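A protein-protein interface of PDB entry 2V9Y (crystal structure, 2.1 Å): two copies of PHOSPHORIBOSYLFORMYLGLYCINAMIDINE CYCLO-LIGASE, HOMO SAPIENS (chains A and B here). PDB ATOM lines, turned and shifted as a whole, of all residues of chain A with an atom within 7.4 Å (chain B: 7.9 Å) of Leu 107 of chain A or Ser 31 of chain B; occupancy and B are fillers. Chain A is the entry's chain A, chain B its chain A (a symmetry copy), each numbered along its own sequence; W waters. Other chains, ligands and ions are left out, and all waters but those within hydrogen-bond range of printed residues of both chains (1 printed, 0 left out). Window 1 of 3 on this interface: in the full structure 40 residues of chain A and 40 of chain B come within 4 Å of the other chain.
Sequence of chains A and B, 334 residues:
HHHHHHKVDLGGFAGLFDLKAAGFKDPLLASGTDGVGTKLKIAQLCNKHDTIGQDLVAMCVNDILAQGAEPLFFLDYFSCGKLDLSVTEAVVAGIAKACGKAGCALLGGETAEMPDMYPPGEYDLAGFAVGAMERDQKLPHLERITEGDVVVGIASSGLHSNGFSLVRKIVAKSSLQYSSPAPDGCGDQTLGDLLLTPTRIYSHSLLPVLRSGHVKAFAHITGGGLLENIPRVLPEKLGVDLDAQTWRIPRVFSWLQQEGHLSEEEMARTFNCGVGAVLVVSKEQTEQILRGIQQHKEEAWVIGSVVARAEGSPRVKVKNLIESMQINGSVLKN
Among the printed residues, pairs that only touch across the chains: Leu 16 of chain A with Leu 28 of chain B, Leu 16 of chain A with Leu 29 of chain B, Leu 16 of chain A with Ala 30 of chain B, Leu 16 of chain A with Gln 67 of chain B, Phe 17 of chain A with Leu 28 of chain B, Asp 18 of chain A with Leu 28 of chain B, Phe 73 of chain A with Ser 31 of chain B, Leu 75 of chain A with Ser 31 of chain B, Leu 75 of chain A with Gly 32 of chain B, Leu 75 of chain A with Thr 33 of chain B, Leu 75 of chain A with Phe 128 of chain B, Asp 76 of chain A with Thr 33 of chain B, Leu 107 of chain A with Ser 31 of chain B and Val 130 of chain A with Val 130 of chain B.
Of the 17 printed residues of chain B, 9 touch a printed residue of chain A. Printed residues of chain B that touch a printed residue of chain A: Leu 28, Leu 29, Ala 30, Ser 31, Gly 32, Thr 33, Gln 67, Phe 128 and Val 130. Hydrophobic or aromatic side chains of chain B within 4 Å of the printed part of chain A: Leu 28, Leu 29, Ala 30, Phe 128 and Val 130. Along chain B the printed residues that touch a printed residue of chain A span positions 28 to 130. Printed residues of chain A that touch a printed residue of chain B: Leu 16, Phe 17, Asp 18, Phe 73, Leu 75, Asp 76, Leu 107 and Val 130. Hydrophobic or aromatic side chains of chain A within 4 Å of the printed part of chain B: Leu 16, Phe 73, Leu 75, Leu 107 and Val 130. Among the printed residues, no Asp or Glu carboxylate lies within 4 Å of a Lys or Arg side-chain nitrogen of the other chain.
Val 130 of chain A touches its own counterpart, Val 130 of chain B. Positions printed for both chains: 73 and 130. Of the 15 pairs that touch across the chains among the printed residues, 1 has its exchanged pair printed and touching as well.
Leu 107 of chain A touches just one residue of chain B: Ser 31 (3.9 Å). Of the printed residues of chain B, Val 130 of chain A touches Val 130 (3.9 Å). Ser 31 of chain B touches just these residues of chain A: Phe 73 (3.3 Å), Leu 75 (3.5 Å) and Leu 107 (3.9 Å). Of the printed residues of chain A, Gln 67 of chain B touches Leu 16. The nearest residue of chain A that does not touch Ser 31 of chain B is Gly 15 of chain A (4.7 Å).
The backbone carbonyl oxygen of Leu 29 of chain B is in hydrogen-bond range of the backbone NH of Phe 17 of chain A (2.8 Å).
Water W1 lies within hydrogen-bond range of O of Gly 15 of chain A (2.5 Å), OE1 of Gln 67 of chain B (2.6 Å) and N of Ser 31 of chain B (3.0 Å).
O of Phe 73 of chain A is in hydrogen-bond range of N of Val 130 of chain A (2.9 Å). The backbone NH of Leu 107 of chain A is in hydrogen-bond range of the backbone carbonyl oxygen of Phe 74 of chain A (2.9 Å). The backbone carbonyl oxygen (O) of Gly 108 of chain A is in hydrogen-bond range of the backbone NH (N) of Asp 76 of chain A (3.4 Å). O of Ala 30 of chain B sits at hydrogen-bond distance from N of Gly 131 of chain B, at 2.8 Å. O of Gly 32 of chain B sits at hydrogen-bond distance from N of Ala 129 of chain B. The backbone carbonyl oxygen of Asp 63 of chain B sits at hydrogen-bond distance from the side-chain amide nitrogen of Gln 67 of chain B (3.4 Å).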
ATOM      1  N   GLY A  15      26.280 -12.604  -3.643  1.00  0.00           N
ATOM      2  CA  GLY A  15      27.614 -13.072  -3.162  1.00  0.00           C
ATOM      3  C   GLY A  15      27.517 -14.049  -1.994  1.00  0.00           C
ATOM      4  O   GLY A  15      26.469 -14.171  -1.354  1.00  0.00           O
ATOM      5  N   LEU A  16      28.613 -14.766  -1.763  1.00  0.00           N
ATOM      6  CA  LEU A  16      28.777 -15.682  -0.632  1.00  0.00           C
ATOM      7  C   LEU A  16      29.651 -15.018   0.421  1.00  0.00           C
ATOM      8  O   LEU A  16      30.653 -14.395   0.078  1.00  0.00           O
ATOM      9  CB  LEU A  16      29.486 -16.960  -1.074  1.00  0.00           C
ATOM     10  CG  LEU A  16      28.884 -17.908  -2.106  1.00  0.00           C
ATOM     11  CD1 LEU A  16      29.977 -18.819  -2.606  1.00  0.00           C
ATOM     12  CD2 LEU A  16      27.740 -18.720  -1.537  1.00  0.00           C
ATOM     13  N   PHE A  17      29.309 -15.174   1.694  1.00  0.00           N
ATOM     14  CA  PHE A  17      30.095 -14.552   2.743  1.00  0.00           C
ATOM     15  C   PHE A  17      31.162 -15.490   3.322  1.00  0.00           C
ATOM     16  O   PHE A  17      30.901 -16.664   3.599  1.00  0.00           O
ATOM     17  CB  PHE A  17      29.179 -13.924   3.825  1.00  0.00           C
ATOM     18  CG  PHE A  17      29.851 -12.848   4.625  1.00  0.00           C
ATOM     19  CD1 PHE A  17      29.758 -11.525   4.244  1.00  0.00           C
ATOM     20  CD2 PHE A  17      30.610 -13.165   5.733  1.00  0.00           C
ATOM     21  CE1 PHE A  17      30.410 -10.529   4.989  1.00  0.00           C
ATOM     22  CE2 PHE A  17      31.274 -12.181   6.462  1.00  0.00           C
ATOM     23  CZ  PHE A  17      31.167 -10.866   6.087  1.00  0.00           C
ATOM     24  N   ASP A  18      32.383 -14.963   3.451  1.00  0.00           N
ATOM     25  CA  ASP A  18      33.549 -15.720   3.881  1.00  0.00           C
ATOM     26  C   ASP A  18      33.856 -15.295   5.323  1.00  0.00           C
ATOM     27  O   ASP A  18      34.472 -14.239   5.550  1.00  0.00           O
ATOM     28  CB  ASP A  18      34.720 -15.420   2.918  1.00  0.00           C
ATOM     29  CG  ASP A  18      35.966 -16.276   3.169  1.00  0.00           C
ATOM     30  OD1 ASP A  18      36.158 -16.827   4.274  1.00  0.00           O
ATOM     31  OD2 ASP A  18      36.792 -16.382   2.240  1.00  0.00           O
ATOM     32  N   LEU A  72      27.048  -8.378   9.283  1.00  0.00           N
ATOM     33  CA  LEU A  72      27.929  -8.816   8.194  1.00  0.00           C
ATOM     34  C   LEU A  72      27.343  -8.431   6.838  1.00  0.00           C
ATOM     35  O   LEU A  72      28.051  -7.968   5.941  1.00  0.00           O
ATOM     36  CB  LEU A  72      28.151 -10.336   8.241  1.00  0.00           C
ATOM     37  CG  LEU A  72      28.684 -10.910   9.557  1.00  0.00           C
ATOM     38  CD1 LEU A  72      28.797 -12.418   9.385  1.00  0.00           C
ATOM     39  CD2 LEU A  72      30.051 -10.306   9.924  1.00  0.00           C
ATOM     40  N   PHE A  73      26.048  -8.669   6.690  1.00  0.00           N
ATOM     41  CA  PHE A  73      25.408  -8.514   5.393  1.00  0.00           C
ATOM     42  C   PHE A  73      23.908  -8.360   5.504  1.00  0.00           C
ATOM     43  O   PHE A  73      23.304  -8.717   6.532  1.00  0.00           O
ATOM     44  CB  PHE A  73      25.834  -9.626   4.393  1.00  0.00           C
ATOM     45  CG  PHE A  73      25.399 -11.030   4.761  1.00  0.00           C
ATOM     46  CD1 PHE A  73      24.099 -11.485   4.460  1.00  0.00           C
ATOM     47  CD2 PHE A  73      26.316 -11.937   5.323  1.00  0.00           C
ATOM     48  CE1 PHE A  73      23.709 -12.810   4.747  1.00  0.00           C
ATOM     49  CE2 PHE A  73      25.940 -13.262   5.613  1.00  0.00           C
ATOM     50  CZ  PHE A  73      24.625 -13.697   5.317  1.00  0.00           C
ATOM     51  N   PHE A  74      23.326  -7.813   4.441  1.00  0.00           N
ATOM     52  CA  PHE A  74      21.934  -7.394   4.432  1.00  0.00           C
ATOM     53  C   PHE A  74      21.297  -7.779   3.072  1.00  0.00           C
ATOM     54  O   PHE A  74      21.962  -7.748   2.047  1.00  0.00           O
ATOM     55  CB  PHE A  74      21.858  -5.874   4.693  1.00  0.00           C
ATOM     56  CG  PHE A  74      20.467  -5.310   4.623  1.00  0.00           C
ATOM     57  CD1 PHE A  74      19.981  -4.771   3.437  1.00  0.00           C
ATOM     58  CD2 PHE A  74      19.641  -5.312   5.748  1.00  0.00           C
ATOM     59  CE1 PHE A  74      18.680  -4.248   3.374  1.00  0.00           C
ATOM     60  CE2 PHE A  74      18.357  -4.829   5.672  1.00  0.00           C
ATOM     61  CZ  PHE A  74      17.877  -4.294   4.491  1.00  0.00           C
ATOM     62  N   LEU A  75      20.025  -8.160   3.098  1.00  0.00           N
ATOM     63  CA  LEU A  75      19.223  -8.421   1.895  1.00  0.00           C
ATOM     64  C   LEU A  75      17.878  -7.747   2.078  1.00  0.00           C
ATOM     65  O   LEU A  75      17.392  -7.654   3.205  1.00  0.00           O
ATOM     66  CB  LEU A  75      19.015  -9.932   1.662  1.00  0.00           C
ATOM     67  CG  LEU A  75      20.208 -10.760   1.112  1.00  0.00           C
ATOM     68  CD1 LEU A  75      21.160 -11.285   2.207  1.00  0.00           C
ATOM     69  CD2 LEU A  75      19.673 -11.936   0.319  1.00  0.00           C
ATOM     70  N   ASP A  76      17.291  -7.255   0.987  1.00  0.00           N
ATOM     71  CA  ASP A  76      15.932  -6.695   1.056  1.00  0.00           C
ATOM     72  C   ASP A  76      14.991  -7.352   0.038  1.00  0.00           C
ATOM     73  O   ASP A  76      15.415  -7.787  -1.047  1.00  0.00           O
ATOM     74  CB  ASP A  76      15.943  -5.185   0.868  1.00  0.00           C
ATOM     75  CG  ASP A  76      16.355  -4.782  -0.532  1.00  0.00           C
ATOM     76  OD1 ASP A  76      15.458  -4.493  -1.362  1.00  0.00           O
ATOM     77  OD2 ASP A  76      17.576  -4.811  -0.803  1.00  0.00           O
ATOM     78  N   CYS A  99      23.691   0.680   3.962  1.00  0.00           N
ATOM     79  CA  CYS A  99      24.581  -0.460   4.152  1.00  0.00           C
ATOM     80  C   CYS A  99      26.043  -0.016   4.311  1.00  0.00           C
ATOM     81  O   CYS A  99      26.725  -0.493   5.228  1.00  0.00           O
ATOM     82  CB  CYS A  99      24.458  -1.470   3.017  1.00  0.00           C
ATOM     83  SG  CYS A  99      22.955  -2.471   3.118  1.00  0.00           S
ATOM     84  N   CYS A 104      28.003  -2.771   6.699  1.00  0.00           N
ATOM     85  CA  CYS A 104      27.703  -4.137   6.230  1.00  0.00           C
ATOM     86  C   CYS A 104      27.502  -4.225   4.721  1.00  0.00           C
ATOM     87  O   CYS A 104      27.160  -3.238   4.080  1.00  0.00           O
ATOM     88  CB  CYS A 104      26.542  -4.770   7.008  1.00  0.00           C
ATOM     89  SG  CYS A 104      24.910  -4.232   6.589  1.00  0.00           S
ATOM     90  N   ALA A 105      27.716  -5.412   4.164  1.00  0.00           N
ATOM     91  CA  ALA A 105      27.579  -5.653   2.747  1.00  0.00           C
ATOM     92  C   ALA A 105      26.118  -5.808   2.340  1.00  0.00           C
ATOM     93  O   ALA A 105      25.343  -6.493   3.007  1.00  0.00           O
ATOM     94  CB  ALA A 105      28.366  -6.908   2.343  1.00  0.00           C
ATOM     95  N   LEU A 106      25.752  -5.160   1.240  1.00  0.00           N
ATOM     96  CA  LEU A 106      24.496  -5.431   0.581  1.00  0.00           C
ATOM     97  C   LEU A 106      24.681  -6.693  -0.275  1.00  0.00           C
ATOM     98  O   LEU A 106      25.279  -6.637  -1.344  1.00  0.00           O
ATOM     99  CB  LEU A 106      24.070  -4.235  -0.273  1.00  0.00           C
ATOM    100  CG  LEU A 106      22.769  -4.417  -1.066  1.00  0.00           C
ATOM    101  CD1 LEU A 106      21.538  -4.671  -0.153  1.00  0.00           C
ATOM    102  CD2 LEU A 106      22.549  -3.221  -1.988  1.00  0.00           C
ATOM    103  N   LEU A 107      24.184  -7.833   0.189  1.00  0.00           N
ATOM    104  CA  LEU A 107      24.486  -9.084  -0.501  1.00  0.00           C
ATOM    105  C   LEU A 107      23.431  -9.546  -1.471  1.00  0.00           C
ATOM    106  O   LEU A 107      23.570 -10.601  -2.079  1.00  0.00           O
ATOM    107  CB  LEU A 107      24.753 -10.214   0.481  1.00  0.00           C
ATOM    108  CG  LEU A 107      26.193 -10.639   0.742  1.00  0.00           C
ATOM    109  CD1 LEU A 107      26.163 -12.071   1.202  1.00  0.00           C
ATOM    110  CD2 LEU A 107      27.072 -10.481  -0.500  1.00  0.00           C
ATOM    111  N   GLY A 108      22.361  -8.791  -1.622  1.00  0.00           N
ATOM    112  CA  GLY A 108      21.305  -9.277  -2.469  1.00  0.00           C
ATOM    113  C   GLY A 108      19.987  -8.625  -2.188  1.00  0.00           C
ATOM    114  O   GLY A 108      19.815  -7.899  -1.219  1.00  0.00           O
ATOM    115  N   GLY A 109      19.046  -8.873  -3.071  1.00  0.00           N
ATOM    116  CA  GLY A 109      17.791  -8.164  -2.972  1.00  0.00           C
ATOM    117  C   GLY A 109      16.882  -8.624  -4.055  1.00  0.00           C
ATOM    118  O   GLY A 109      17.313  -9.307  -4.996  1.00  0.00           O
ATOM    119  N   VAL A 130      22.301 -10.367   8.680  1.00  0.00           N
ATOM    120  CA  VAL A 130      22.981 -11.431   9.401  1.00  0.00           C
ATOM    121  C   VAL A 130      24.238 -10.850  10.026  1.00  0.00           C
ATOM    122  O   VAL A 130      24.972 -10.083   9.377  1.00  0.00           O
ATOM    123  CB  VAL A 130      23.333 -12.665   8.500  1.00  0.00           C
ATOM    124  CG1 VAL A 130      24.198 -13.648   9.260  1.00  0.00           C
ATOM    125  CG2 VAL A 130      22.061 -13.359   8.030  1.00  0.00           C
ATOM    126  N   LEU B  28      31.504 -21.339   3.820  1.00  0.00           N
ATOM    127  CA  LEU B  28      31.044 -20.096   3.194  1.00  0.00           C
ATOM    128  C   LEU B  28      29.559 -20.023   3.429  1.00  0.00           C
ATOM    129  O   LEU B  28      28.893 -21.060   3.484  1.00  0.00           O
ATOM    130  CB  LEU B  28      31.298 -20.075   1.682  1.00  0.00           C
ATOM    131  CG  LEU B  28      32.725 -20.240   1.165  1.00  0.00           C
ATOM    132  CD1 LEU B  28      32.679 -20.278  -0.353  1.00  0.00           C
ATOM    133  CD2 LEU B  28      33.626 -19.129   1.670  1.00  0.00           C
ATOM    134  N   LEU B  29      29.032 -18.805   3.551  1.00  0.00           N
ATOM    135  CA  LEU B  29      27.586 -18.609   3.746  1.00  0.00           C
ATOM    136  C   LEU B  29      26.909 -18.130   2.472  1.00  0.00           C
ATOM    137  O   LEU B  29      27.378 -17.171   1.851  1.00  0.00           O
ATOM    138  CB  LEU B  29      27.325 -17.601   4.877  1.00  0.00           C
ATOM    139  CG  LEU B  29      27.875 -17.863   6.289  1.00  0.00           C
ATOM    140  CD1 LEU B  29      27.630 -16.635   7.164  1.00  0.00           C
ATOM    141  CD2 LEU B  29      27.251 -19.115   6.907  1.00  0.00           C
ATOM    142  N   ALA B  30      25.830 -18.803   2.086  1.00  0.00           N
ATOM    143  CA  ALA B  30      24.968 -18.357   0.992  1.00  0.00           C
ATOM    144  C   ALA B  30      23.653 -17.826   1.554  1.00  0.00           C
ATOM    145  O   ALA B  30      23.156 -18.315   2.577  1.00  0.00           O
ATOM    146  CB  ALA B  30      24.692 -19.484  -0.014  1.00  0.00           C
ATOM    147  N   SER B  31      23.105 -16.804   0.905  1.00  0.00           N
ATOM    148  CA  SER B  31      21.819 -16.276   1.328  1.00  0.00           C
ATOM    149  C   SER B  31      20.980 -15.820   0.146  1.00  0.00           C
ATOM    150  O   SER B  31      21.491 -15.538  -0.937  1.00  0.00           O
ATOM    151  CB  SER B  31      21.981 -15.140   2.319  1.00  0.00           C
ATOM    152  OG  SER B  31      23.010 -14.275   1.895  1.00  0.00           O
ATOM    153  N   GLY B  32      19.682 -15.764   0.368  1.00  0.00           N
ATOM    154  CA  GLY B  32      18.783 -15.299  -0.658  1.00  0.00           C
ATOM    155  C   GLY B  32      17.442 -14.954  -0.064  1.00  0.00           C
ATOM    156  O   GLY B  32      17.066 -15.451   1.010  1.00  0.00           O
ATOM    157  N   THR B  33      16.755 -14.070  -0.766  1.00  0.00           N
ATOM    158  CA  THR B  33      15.412 -13.670  -0.412  1.00  0.00           C
ATOM    159  C   THR B  33      14.530 -13.996  -1.603  1.00  0.00           C
ATOM    160  O   THR B  33      14.965 -13.924  -2.770  1.00  0.00           O
ATOM    161  CB  THR B  33      15.326 -12.169  -0.013  1.00  0.00           C
ATOM    162  OG1 THR B  33      13.992 -11.850   0.358  1.00  0.00           O
ATOM    163  CG2 THR B  33      15.795 -11.208  -1.163  1.00  0.00           C
ATOM    164  N   CYS B  60      13.040 -20.095  -1.338  1.00  0.00           N
ATOM    165  CA  CYS B  60      14.296 -19.631  -0.708  1.00  0.00           C
ATOM    166  C   CYS B  60      15.357 -20.740  -0.606  1.00  0.00           C
ATOM    167  O   CYS B  60      16.519 -20.518  -0.917  1.00  0.00           O
ATOM    168  CB  CYS B  60      14.038 -18.999   0.680  1.00  0.00           C
ATOM    169  SG  CYS B  60      12.945 -17.583   0.584  1.00  0.00           S
ATOM    170  N   ASP B  63      16.828 -21.885  -4.021  1.00  0.00           N
ATOM    171  CA  ASP B  63      17.705 -20.812  -4.476  1.00  0.00           C
ATOM    172  C   ASP B  63      19.106 -20.878  -3.893  1.00  0.00           C
ATOM    173  O   ASP B  63      20.072 -20.628  -4.581  1.00  0.00           O
ATOM    174  CB  ASP B  63      17.097 -19.432  -4.195  1.00  0.00           C
ATOM    175  CG  ASP B  63      16.099 -18.980  -5.287  1.00  0.00           C
ATOM    176  OD1 ASP B  63      15.935 -19.633  -6.342  1.00  0.00           O
ATOM    177  OD2 ASP B  63      15.475 -17.944  -5.063  1.00  0.00           O
ATOM    178  N   ILE B  64      19.240 -21.184  -2.619  1.00  0.00           N
ATOM    179  CA  ILE B  64      20.589 -21.316  -2.073  1.00  0.00           C
ATOM    180  C   ILE B  64      21.231 -22.676  -2.376  1.00  0.00           C
ATOM    181  O   ILE B  64      22.451 -22.758  -2.482  1.00  0.00           O
ATOM    182  CB  ILE B  64      20.689 -20.996  -0.561  1.00  0.00           C
ATOM    183  CG1 ILE B  64      19.779 -21.898   0.272  1.00  0.00           C
ATOM    184  CG2 ILE B  64      20.451 -19.472  -0.284  1.00  0.00           C
ATOM    185  CD1 ILE B  64      19.906 -21.621   1.794  1.00  0.00           C
ATOM    186  N   GLN B  67      23.677 -22.584  -5.181  1.00  0.00           N
ATOM    187  CA  GLN B  67      25.039 -22.135  -4.917  1.00  0.00           C
ATOM    188  C   GLN B  67      25.859 -23.254  -4.261  1.00  0.00           C
ATOM    189  O   GLN B  67      27.048 -23.114  -4.036  1.00  0.00           O
ATOM    190  CB  GLN B  67      25.010 -20.840  -4.066  1.00  0.00           C
ATOM    191  CG  GLN B  67      24.031 -19.745  -4.641  1.00  0.00           C
ATOM    192  CD  GLN B  67      23.662 -18.622  -3.657  1.00  0.00           C
ATOM    193  OE1 GLN B  67      24.536 -17.958  -3.086  1.00  0.00           O
ATOM    194  NE2 GLN B  67      22.350 -18.383  -3.480  1.00  0.00           N
ATOM    195  N   ALA B  69      24.868 -24.753  -1.339  1.00  0.00           N
ATOM    196  CA  ALA B  69      24.693 -24.648   0.113  1.00  0.00           C
ATOM    197  C   ALA B  69      23.600 -25.541   0.678  1.00  0.00           C
ATOM    198  O   ALA B  69      22.539 -25.726   0.066  1.00  0.00           O
ATOM    199  CB  ALA B  69      24.437 -23.160   0.523  1.00  0.00           C
ATOM    200  N   PHE B  73      18.866 -22.128   8.073  1.00  0.00           N
ATOM    201  CA  PHE B  73      17.799 -21.433   8.775  1.00  0.00           C
ATOM    202  C   PHE B  73      17.053 -20.469   7.881  1.00  0.00           C
ATOM    203  O   PHE B  73      17.557 -20.063   6.819  1.00  0.00           O
ATOM    204  CB  PHE B  73      18.294 -20.780  10.097  1.00  0.00           C
ATOM    205  CG  PHE B  73      19.302 -19.661   9.929  1.00  0.00           C
ATOM    206  CD1 PHE B  73      18.880 -18.349   9.629  1.00  0.00           C
ATOM    207  CD2 PHE B  73      20.670 -19.891  10.163  1.00  0.00           C
ATOM    208  CE1 PHE B  73      19.810 -17.293   9.530  1.00  0.00           C
ATOM    209  CE2 PHE B  73      21.607 -18.846  10.069  1.00  0.00           C
ATOM    210  CZ  PHE B  73      21.167 -17.537   9.753  1.00  0.00           C
ATOM    211  N   PHE B 128      13.565 -15.382   3.741  1.00  0.00           N
ATOM    212  CA  PHE B 128      15.019 -15.245   3.752  1.00  0.00           C
ATOM    213  C   PHE B 128      15.566 -16.575   4.264  1.00  0.00           C
ATOM    214  O   PHE B 128      15.128 -17.057   5.307  1.00  0.00           O
ATOM    215  CB  PHE B 128      15.473 -14.117   4.706  1.00  0.00           C
ATOM    216  CG  PHE B 128      14.791 -12.766   4.474  1.00  0.00           C
ATOM    217  CD1 PHE B 128      15.332 -11.846   3.584  1.00  0.00           C
ATOM    218  CD2 PHE B 128      13.630 -12.415   5.182  1.00  0.00           C
ATOM    219  CE1 PHE B 128      14.731 -10.605   3.368  1.00  0.00           C
ATOM    220  CE2 PHE B 128      13.010 -11.178   4.975  1.00  0.00           C
ATOM    221  CZ  PHE B 128      13.568 -10.264   4.060  1.00  0.00           C
ATOM    222  N   ALA B 129      16.534 -17.142   3.555  1.00  0.00           N
ATOM    223  CA  ALA B 129      17.193 -18.381   3.991  1.00  0.00           C
ATOM    224  C   ALA B 129      18.717 -18.208   3.981  1.00  0.00           C
ATOM    225  O   ALA B 129      19.278 -17.484   3.134  1.00  0.00           O
ATOM    226  CB  ALA B 129      16.760 -19.559   3.118  1.00  0.00           C
ATOM    227  N   VAL B 130      19.388 -18.824   4.960  1.00  0.00           N
ATOM    228  CA  VAL B 130      20.842 -18.824   4.982  1.00  0.00           C
ATOM    229  C   VAL B 130      21.317 -20.266   4.962  1.00  0.00           C
ATOM    230  O   VAL B 130      20.767 -21.125   5.675  1.00  0.00           O
ATOM    231  CB  VAL B 130      21.443 -18.063   6.215  1.00  0.00           C
ATOM    232  CG1 VAL B 130      22.943 -18.258   6.281  1.00  0.00           C
ATOM    233  CG2 VAL B 130      21.122 -16.576   6.130  1.00  0.00           C
ATOM    234  N   GLY B 131      22.337 -20.510   4.152  1.00  0.00           N
ATOM    235  CA  GLY B 131      22.949 -21.826   4.031  1.00  0.00           C
ATOM    236  C   GLY B 131      24.453 -21.747   4.108  1.00  0.00           C
ATOM    237  O   GLY B 131      25.030 -20.665   4.188  1.00  0.00           O
ATOM    238  N   ALA B 132      25.088 -22.912   4.081  1.00  0.00           N
ATOM    239  CA  ALA B 132      26.532 -23.006   4.250  1.00  0.00           C
ATOM    240  C   ALA B 132      27.035 -24.247   3.539  1.00  0.00           C
ATOM    241  O   ALA B 132      26.304 -25.224   3.349  1.00  0.00           O
ATOM    242  CB  ALA B 132      26.909 -23.048   5.715  1.00  0.00           C
HETATM  243  O   HOH W   1      24.744 -16.017  -1.434  1.00  0.00           O
